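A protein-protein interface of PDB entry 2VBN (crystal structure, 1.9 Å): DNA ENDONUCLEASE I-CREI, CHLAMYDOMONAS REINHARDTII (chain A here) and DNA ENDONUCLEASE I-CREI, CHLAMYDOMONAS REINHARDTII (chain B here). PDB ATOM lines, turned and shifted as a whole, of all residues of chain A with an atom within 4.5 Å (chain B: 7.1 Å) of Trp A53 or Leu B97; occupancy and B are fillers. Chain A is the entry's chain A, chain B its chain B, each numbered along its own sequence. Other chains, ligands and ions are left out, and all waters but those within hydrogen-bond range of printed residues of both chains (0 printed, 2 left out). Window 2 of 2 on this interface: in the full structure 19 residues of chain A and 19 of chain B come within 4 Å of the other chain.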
ATOM      1  N   PHE A  16      -3.820  22.348  20.226  1.00  0.00           N
ATOM      2  CA  PHE A  16      -3.988  21.017  20.795  1.00  0.00           C
ATOM      3  C   PHE A  16      -2.966  20.769  21.915  1.00  0.00           C
ATOM      4  O   PHE A  16      -3.285  20.156  22.955  1.00  0.00           O
ATOM      5  CB  PHE A  16      -3.888  19.920  19.730  1.00  0.00           C
ATOM      6  CG  PHE A  16      -4.342  18.573  20.246  1.00  0.00           C
ATOM      7  CD1 PHE A  16      -5.700  18.277  20.294  1.00  0.00           C
ATOM      8  CD2 PHE A  16      -3.432  17.657  20.772  1.00  0.00           C
ATOM      9  CE1 PHE A  16      -6.152  17.069  20.781  1.00  0.00           C
ATOM     10  CE2 PHE A  16      -3.879  16.423  21.268  1.00  0.00           C
ATOM     11  CZ  PHE A  16      -5.247  16.138  21.271  1.00  0.00           C
ATOM     12  N   GLN A  47      -3.191  11.064  25.016  1.00  0.00           N
ATOM     13  CA  GLN A  47      -4.545  10.798  24.586  1.00  0.00           C
ATOM     14  C   GLN A  47      -4.905   9.350  24.912  1.00  0.00           C
ATOM     15  O   GLN A  47      -4.078   8.426  24.833  1.00  0.00           O
ATOM     16  CB  GLN A  47      -4.717  11.072  23.081  1.00  0.00           C
ATOM     17  CG  GLN A  47      -6.163  11.321  22.629  1.00  0.00           C
ATOM     18  CD  GLN A  47      -6.750  12.670  23.045  1.00  0.00           C
ATOM     19  OE1 GLN A  47      -7.938  12.904  22.840  1.00  0.00           O
ATOM     20  NE2 GLN A  47      -5.942  13.555  23.626  1.00  0.00           N
ATOM     21  N   GLN A  50      -7.772   4.566  22.668  1.00  0.00           N
ATOM     22  CA  GLN A  50      -8.715   4.458  21.563  1.00  0.00           C
ATOM     23  C   GLN A  50      -8.482   5.510  20.451  1.00  0.00           C
ATOM     24  O   GLN A  50      -8.875   5.300  19.295  1.00  0.00           O
ATOM     25  CB  GLN A  50     -10.178   4.368  22.049  1.00  0.00           C
ATOM     26  CG  GLN A  50     -10.869   5.695  22.256  1.00  0.00           C
ATOM     27  CD  GLN A  50     -12.379   5.605  22.568  1.00  0.00           C
ATOM     28  OE1 GLN A  50     -12.762   5.259  23.676  1.00  0.00           O
ATOM     29  NE2 GLN A  50     -13.227   5.970  21.607  1.00  0.00           N
ATOM     30  N   ARG A  51      -7.809   6.618  20.779  1.00  0.00           N
ATOM     31  CA  ARG A  51      -7.467   7.700  19.829  1.00  0.00           C
ATOM     32  C   ARG A  51      -5.966   7.775  19.474  1.00  0.00           C
ATOM     33  O   ARG A  51      -5.418   8.821  19.079  1.00  0.00           O
ATOM     34  CB  ARG A  51      -7.959   9.072  20.354  1.00  0.00           C
ATOM     35  CG  ARG A  51      -9.507   9.272  20.291  1.00  0.00           C
ATOM     36  CD  ARG A  51      -9.995  10.638  20.855  1.00  0.00           C
ATOM     37  NE  ARG A  51      -9.755  10.863  22.278  1.00  0.00           N
ATOM     38  CZ  ARG A  51     -10.581  10.460  23.247  1.00  0.00           C
ATOM     39  NH1 ARG A  51     -11.667   9.768  22.939  1.00  0.00           N
ATOM     40  NH2 ARG A  51     -10.316  10.723  24.527  1.00  0.00           N
ATOM     41  N   ARG A  52      -5.299   6.642  19.607  1.00  0.00           N
ATOM     42  CA  ARG A  52      -3.866   6.562  19.397  1.00  0.00           C
ATOM     43  C   ARG A  52      -3.533   6.904  17.933  1.00  0.00           C
ATOM     44  O   ARG A  52      -2.473   7.455  17.643  1.00  0.00           O
ATOM     45  CB  ARG A  52      -3.360   5.168  19.783  1.00  0.00           C
ATOM     46  CG  ARG A  52      -1.839   5.077  19.653  1.00  0.00           C
ATOM     47  CD  ARG A  52      -1.348   3.660  19.627  1.00  0.00           C
ATOM     48  NE  ARG A  52      -0.070   3.631  18.919  1.00  0.00           N
ATOM     49  CZ  ARG A  52       1.039   3.093  19.393  1.00  0.00           C
ATOM     50  NH1 ARG A  52       1.033   2.540  20.603  1.00  0.00           N
ATOM     51  NH2 ARG A  52       2.143   3.089  18.644  1.00  0.00           N
ATOM     52  N   TRP A  53      -4.466   6.631  17.024  1.00  0.00           N
ATOM     53  CA  TRP A  53      -4.281   7.012  15.611  1.00  0.00           C
ATOM     54  C   TRP A  53      -3.832   8.473  15.450  1.00  0.00           C
ATOM     55  O   TRP A  53      -2.991   8.793  14.596  1.00  0.00           O
ATOM     56  CB  TRP A  53      -5.541   6.720  14.788  1.00  0.00           C
ATOM     57  CG  TRP A  53      -6.689   7.645  15.068  1.00  0.00           C
ATOM     58  CD1 TRP A  53      -7.734   7.428  15.953  1.00  0.00           C
ATOM     59  CD2 TRP A  53      -6.901   8.936  14.499  1.00  0.00           C
ATOM     60  NE1 TRP A  53      -8.576   8.509  15.944  1.00  0.00           N
ATOM     61  CE2 TRP A  53      -8.094   9.448  15.064  1.00  0.00           C
ATOM     62  CE3 TRP A  53      -6.209   9.710  13.553  1.00  0.00           C
ATOM     63  CZ2 TRP A  53      -8.606  10.699  14.709  1.00  0.00           C
ATOM     64  CZ3 TRP A  53      -6.706  10.951  13.215  1.00  0.00           C
ATOM     65  CH2 TRP A  53      -7.901  11.435  13.787  1.00  0.00           C
ATOM     66  N   PHE A  54      -4.386   9.347  16.289  1.00  0.00           N
ATOM     67  CA  PHE A  54      -4.077  10.782  16.255  1.00  0.00           C
ATOM     68  C   PHE A  54      -2.617  11.018  16.634  1.00  0.00           C
ATOM     69  O   PHE A  54      -1.943  11.863  16.035  1.00  0.00           O
ATOM     70  CB  PHE A  54      -5.032  11.478  17.227  1.00  0.00           C
ATOM     71  CG  PHE A  54      -4.890  12.984  17.281  1.00  0.00           C
ATOM     72  CD1 PHE A  54      -3.968  13.572  18.131  1.00  0.00           C
ATOM     73  CD2 PHE A  54      -5.692  13.810  16.499  1.00  0.00           C
ATOM     74  CE1 PHE A  54      -3.857  14.955  18.215  1.00  0.00           C
ATOM     75  CE2 PHE A  54      -5.583  15.209  16.574  1.00  0.00           C
ATOM     76  CZ  PHE A  54      -4.672  15.773  17.436  1.00  0.00           C
ATOM     77  N   LEU A  55      -2.125  10.265  17.629  1.00  0.00           N
ATOM     78  CA  LEU A  55      -0.712  10.337  18.041  1.00  0.00           C
ATOM     79  C   LEU A  55       0.258   9.725  17.025  1.00  0.00           C
ATOM     80  O   LEU A  55       1.300  10.322  16.700  1.00  0.00           O
ATOM     81  CB  LEU A  55      -0.504   9.715  19.436  1.00  0.00           C
ATOM     82  CG  LEU A  55      -1.457  10.224  20.554  1.00  0.00           C
ATOM     83  CD1 LEU A  55      -1.162   9.485  21.934  1.00  0.00           C
ATOM     84  CD2 LEU A  55      -1.265  11.773  20.751  1.00  0.00           C
ATOM     85  N   ASP A  56      -0.110   8.561  16.491  1.00  0.00           N
ATOM     86  CA  ASP A  56       0.671   7.930  15.404  1.00  0.00           C
ATOM     87  C   ASP A  56       0.835   8.882  14.223  1.00  0.00           C
ATOM     88  O   ASP A  56       1.936   9.045  13.693  1.00  0.00           O
ATOM     89  CB  ASP A  56       0.042   6.600  14.935  1.00  0.00           C
ATOM     90  CG  ASP A  56       0.069   5.503  16.002  1.00  0.00           C
ATOM     91  OD1 ASP A  56       0.965   5.447  16.871  1.00  0.00           O
ATOM     92  OD2 ASP A  56      -0.844   4.648  15.962  1.00  0.00           O
ATOM     93  N   LYS A  57      -0.251   9.532  13.815  1.00  0.00           N
ATOM     94  CA  LYS A  57      -0.167  10.591  12.801  1.00  0.00           C
ATOM     95  C   LYS A  57       0.825  11.684  13.147  1.00  0.00           C
ATOM     96  O   LYS A  57       1.527  12.169  12.278  1.00  0.00           O
ATOM     97  CB  LYS A  57      -1.546  11.228  12.553  1.00  0.00           C
ATOM     98  CG  LYS A  57      -1.786  11.751  11.187  1.00  0.00           C
ATOM     99  CD  LYS A  57      -3.277  11.740  10.940  1.00  0.00           C
ATOM    100  CE  LYS A  57      -3.679  12.988  10.195  1.00  0.00           C
ATOM    101  NZ  LYS A  57      -2.817  13.216   9.008  1.00  0.00           N
ATOM    102  N   ALA B  14      -9.663  25.354  17.338  1.00  0.00           N
ATOM    103  CA  ALA B  14     -10.079  23.973  17.025  1.00  0.00           C
ATOM    104  C   ALA B  14      -9.156  22.956  17.720  1.00  0.00           C
ATOM    105  O   ALA B  14      -9.609  21.916  18.271  1.00  0.00           O
ATOM    106  CB  ALA B  14     -10.093  23.759  15.503  1.00  0.00           C
ATOM    107  N   VAL B  17      -9.894  23.246  21.517  1.00  0.00           N
ATOM    108  CA  VAL B  17     -11.147  22.525  21.759  1.00  0.00           C
ATOM    109  C   VAL B  17     -11.005  20.993  21.663  1.00  0.00           C
ATOM    110  O   VAL B  17     -11.499  20.246  22.527  1.00  0.00           O
ATOM    111  CB  VAL B  17     -12.226  23.062  20.769  1.00  0.00           C
ATOM    112  CG1 VAL B  17     -13.374  22.189  20.729  1.00  0.00           C
ATOM    113  CG2 VAL B  17     -12.617  24.459  21.174  1.00  0.00           C
ATOM    114  N   ASP B  18     -10.345  20.502  20.616  1.00  0.00           N
ATOM    115  CA  ASP B  18     -10.109  19.065  20.524  1.00  0.00           C
ATOM    116  C   ASP B  18      -9.353  18.565  21.787  1.00  0.00           C
ATOM    117  O   ASP B  18      -9.486  17.413  22.180  1.00  0.00           O
ATOM    118  CB  ASP B  18      -9.316  18.723  19.234  1.00  0.00           C
ATOM    119  CG  ASP B  18     -10.224  18.494  18.006  1.00  0.00           C
ATOM    120  OD1 ASP B  18     -11.478  18.366  18.185  1.00  0.00           O
ATOM    121  OD2 ASP B  18      -9.673  18.414  16.863  1.00  0.00           O
ATOM    122  N   GLY B  19      -8.524  19.395  22.413  1.00  0.00           N
ATOM    123  CA  GLY B  19      -7.870  19.050  23.678  1.00  0.00           C
ATOM    124  C   GLY B  19      -8.747  19.201  24.931  1.00  0.00           C
ATOM    125  O   GLY B  19      -9.147  18.174  25.513  1.00  0.00           O
ATOM    126  N   PHE B  94     -12.189  22.732  11.042  1.00  0.00           N
ATOM    127  CA  PHE B  94     -10.824  22.624  11.573  1.00  0.00           C
ATOM    128  C   PHE B  94     -10.699  21.604  12.700  1.00  0.00           C
ATOM    129  O   PHE B  94      -9.591  21.318  13.165  1.00  0.00           O
ATOM    130  CB  PHE B  94     -10.342  24.001  12.047  1.00  0.00           C
ATOM    131  CG  PHE B  94     -10.441  25.038  10.978  1.00  0.00           C
ATOM    132  CD1 PHE B  94      -9.684  24.894   9.802  1.00  0.00           C
ATOM    133  CD2 PHE B  94     -11.331  26.109  11.093  1.00  0.00           C
ATOM    134  CE1 PHE B  94      -9.811  25.822   8.764  1.00  0.00           C
ATOM    135  CE2 PHE B  94     -11.449  27.059  10.058  1.00  0.00           C
ATOM    136  CZ  PHE B  94     -10.695  26.904   8.889  1.00  0.00           C
ATOM    137  N   LEU B  95     -11.839  21.084  13.159  1.00  0.00           N
ATOM    138  CA  LEU B  95     -11.845  20.103  14.231  1.00  0.00           C
ATOM    139  C   LEU B  95     -11.424  18.763  13.633  1.00  0.00           C
ATOM    140  O   LEU B  95     -11.753  18.514  12.478  1.00  0.00           O
ATOM    141  CB  LEU B  95     -13.248  20.006  14.853  1.00  0.00           C
ATOM    142  CG  LEU B  95     -13.714  21.216  15.672  1.00  0.00           C
ATOM    143  CD1 LEU B  95     -15.144  20.959  16.123  1.00  0.00           C
ATOM    144  CD2 LEU B  95     -12.808  21.420  16.910  1.00  0.00           C
ATOM    145  N   LYS B  96     -10.667  17.957  14.387  1.00  0.00           N
ATOM    146  CA  LYS B  96     -10.229  16.624  13.968  1.00  0.00           C
ATOM    147  C   LYS B  96     -10.764  15.529  14.890  1.00  0.00           C
ATOM    148  O   LYS B  96     -10.963  14.389  14.448  1.00  0.00           O
ATOM    149  CB  LYS B  96      -8.704  16.515  14.033  1.00  0.00           C
ATOM    150  CG  LYS B  96      -7.953  17.568  13.195  1.00  0.00           C
ATOM    151  CD  LYS B  96      -6.475  17.350  13.243  1.00  0.00           C
ATOM    152  CE  LYS B  96      -5.849  18.244  12.201  1.00  0.00           C
ATOM    153  NZ  LYS B  96      -4.383  18.134  12.298  1.00  0.00           N
ATOM    154  N   LEU B  97     -10.919  15.834  16.177  1.00  0.00           N
ATOM    155  CA  LEU B  97     -11.420  14.839  17.133  1.00  0.00           C
ATOM    156  C   LEU B  97     -12.905  14.999  17.447  1.00  0.00           C
ATOM    157  O   LEU B  97     -13.594  13.997  17.701  1.00  0.00           O
ATOM    158  CB  LEU B  97     -10.633  14.858  18.447  1.00  0.00           C
ATOM    159  CG  LEU B  97      -9.151  14.462  18.419  1.00  0.00           C
ATOM    160  CD1 LEU B  97      -8.540  14.368  19.849  1.00  0.00           C
ATOM    161  CD2 LEU B  97      -8.985  13.164  17.635  1.00  0.00           C
ATOM    162  N   LYS B  98     -13.405  16.238  17.426  1.00  0.00           N
ATOM    163  CA  LYS B  98     -14.796  16.503  17.827  1.00  0.00           C
ATOM    164  C   LYS B  98     -15.642  17.052  16.661  1.00  0.00           C
ATOM    165  O   LYS B  98     -16.747  17.587  16.850  1.00  0.00           O
ATOM    166  CB  LYS B  98     -14.843  17.444  19.036  1.00  0.00           C
ATOM    167  CG  LYS B  98     -14.107  16.923  20.262  1.00  0.00           C
ATOM    168  CD  LYS B  98     -13.969  18.036  21.350  1.00  0.00           C
ATOM    169  CE  LYS B  98     -13.106  17.538  22.545  1.00  0.00           C
ATOM    170  NZ  LYS B  98     -13.866  16.629  23.486  1.00  0.00           N
ATOM    171  N   GLN B  99     -15.134  16.869  15.441  1.00  0.00           N
ATOM    172  CA  GLN B  99     -15.860  17.325  14.261  1.00  0.00           C
ATOM    173  C   GLN B  99     -17.247  16.676  14.115  1.00  0.00           C
ATOM    174  O   GLN B  99     -18.253  17.342  13.794  1.00  0.00           O
ATOM    175  CB  GLN B  99     -15.000  17.116  13.010  1.00  0.00           C
ATOM    176  CG  GLN B  99     -15.560  17.817  11.773  1.00  0.00           C
ATOM    177  CD  GLN B  99     -14.716  17.526  10.557  1.00  0.00           C
ATOM    178  OE1 GLN B  99     -14.547  16.366  10.187  1.00  0.00           O
ATOM    179  NE2 GLN B  99     -14.129  18.558   9.968  1.00  0.00           N
ATOM    180  N   LYS B 100     -17.337  15.376  14.396  1.00  0.00           N
ATOM    181  CA  LYS B 100     -18.614  14.726  14.209  1.00  0.00           C
ATOM    182  C   LYS B 100     -19.630  15.237  15.226  1.00  0.00           C
ATOM    183  O   LYS B 100     -20.816  15.453  14.898  1.00  0.00           O
ATOM    184  CB  LYS B 100     -18.478  13.204  14.304  1.00  0.00           C
ATOM    185  CG  LYS B 100     -17.919  12.521  13.057  1.00  0.00           C
ATOM    186  CD  LYS B 100     -17.782  11.054  13.450  1.00  0.00           C
ATOM    187  CE  LYS B 100     -17.354  10.124  12.344  1.00  0.00           C
ATOM    188  NZ  LYS B 100     -17.038   8.794  12.982  1.00  0.00           N
ATOM    189  N   GLN B 101     -19.174  15.416  16.459  1.00  0.00           N
ATOM    190  CA  GLN B 101     -20.082  15.912  17.499  1.00  0.00           C
ATOM    191  C   GLN B 101     -20.555  17.299  17.074  1.00  0.00           C
ATOM    192  O   GLN B 101     -21.729  17.586  17.168  1.00  0.00           O
ATOM    193  CB  GLN B 101     -19.383  16.031  18.866  1.00  0.00           C
ATOM    194  CG  GLN B 101     -19.036  14.679  19.538  1.00  0.00           C
ATOM    195  CD  GLN B 101     -17.599  14.222  19.283  1.00  0.00           C
ATOM    196  OE1 GLN B 101     -17.109  14.281  18.143  1.00  0.00           O
ATOM    197  NE2 GLN B 101     -16.924  13.736  20.333  1.00  0.00           N
ATOM    198  N   LEU B 135     -19.897   9.278  20.782  1.00  0.00           N
ATOM    199  CA  LEU B 135     -18.613   9.846  20.363  1.00  0.00           C
ATOM    200  C   LEU B 135     -17.755  10.438  21.491  1.00  0.00           C
ATOM    201  O   LEU B 135     -16.522  10.286  21.481  1.00  0.00           O
ATOM    202  CB  LEU B 135     -18.847  10.907  19.292  1.00  0.00           C
ATOM    203  CG  LEU B 135     -19.399  10.280  18.020  1.00  0.00           C
ATOM    204  CD1 LEU B 135     -20.184  11.339  17.248  1.00  0.00           C
ATOM    205  CD2 LEU B 135     -18.270   9.666  17.190  1.00  0.00           C
ATOM    206  N   ASN B 136     -18.387  11.143  22.426  1.00  0.00           N
ATOM    207  CA  ASN B 136     -17.715  11.597  23.652  1.00  0.00           C
ATOM    208  C   ASN B 136     -17.239  10.444  24.498  1.00  0.00           C
ATOM    209  O   ASN B 136     -17.659   9.301  24.282  1.00  0.00           O
ATOM    210  CB  ASN B 136     -18.652  12.500  24.472  1.00  0.00           C
ATOM    211  CG  ASN B 136     -18.982  13.785  23.708  1.00  0.00           C
ATOM    212  OD1 ASN B 136     -18.307  14.117  22.733  1.00  0.00           O
ATOM    213  ND2 ASN B 136     -20.048  14.454  24.084  1.00  0.00           N
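Among the printed residues, pairs that only touch across the chains: Gln A47 with Leu B97 (3.4 Å), Phe A54 with Leu B97 (3.5 Å), Phe A16 with Asp B18 (3.6 Å), Phe A16 with Gly B19 (3.7 Å), Phe A16 with Leu B97 (3.7 Å) and Trp A53 with Leu B97 (3.8 Å).
The side-chain amide oxygen of Gln A47 is in hydrogen-bond range of the guanidinium group of Arg A51 (2.8 Å).
The backbone NH of Lys B96 sits at hydrogen-bond distance from the side-chain carboxylate of Asp B18 (2.7 Å).
OD2 of Asp B18 lies within hydrogen-bond range of N of Leu B97 (2.9 Å).
OD1 of Asp B18 sits at hydrogen-bond distance from N of Lys B98, at 3.0 Å.
Printed residues of chain B within 4 Å of Phe A16: Asp B18, Gly B19 and Leu B97.
Printed residues of chain B within 4 Å of Gln A47: Leu B97 (3.4 Å).
Arg A52 touches none of the printed residues of chain B.
Of chain B, only Leu B97 (3.8 Å) comes within 4 Å of Trp A53.
Of the printed residues of chain B, Phe A54 touches Leu B97 (3.5 Å).
Of the printed residues of chain A, Asp B18 touches Phe A16.
Of the printed residues of chain A, Gly B19 touches Phe A16.
Leu B97 touches just these residues of chain A: Phe A16 (3.7 Å), Gln A47 (3.4 Å), Trp A53 (3.8 Å) and Phe A54 (3.5 Å).
The nearest residue of chain A that does not touch Leu B97 is Arg A51 (4.1 Å).
The nearest printed residue of chain B that does not touch Phe A54 is Lys B96 (4.1 Å).
Of the 10 printed residues of chain A, 4 touch a printed residue of chain B.
Hydrophobic or aromatic side chains of chain A that line the printed part of chain B: Phe A16, Trp A53 and Phe A54.
Among the printed residues, 6 pairs touch across the chains.
Among the printed residues, no Asp or Glu carboxylate lies within 4 Å of a Lys or Arg side-chain nitrogen of the other chain.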
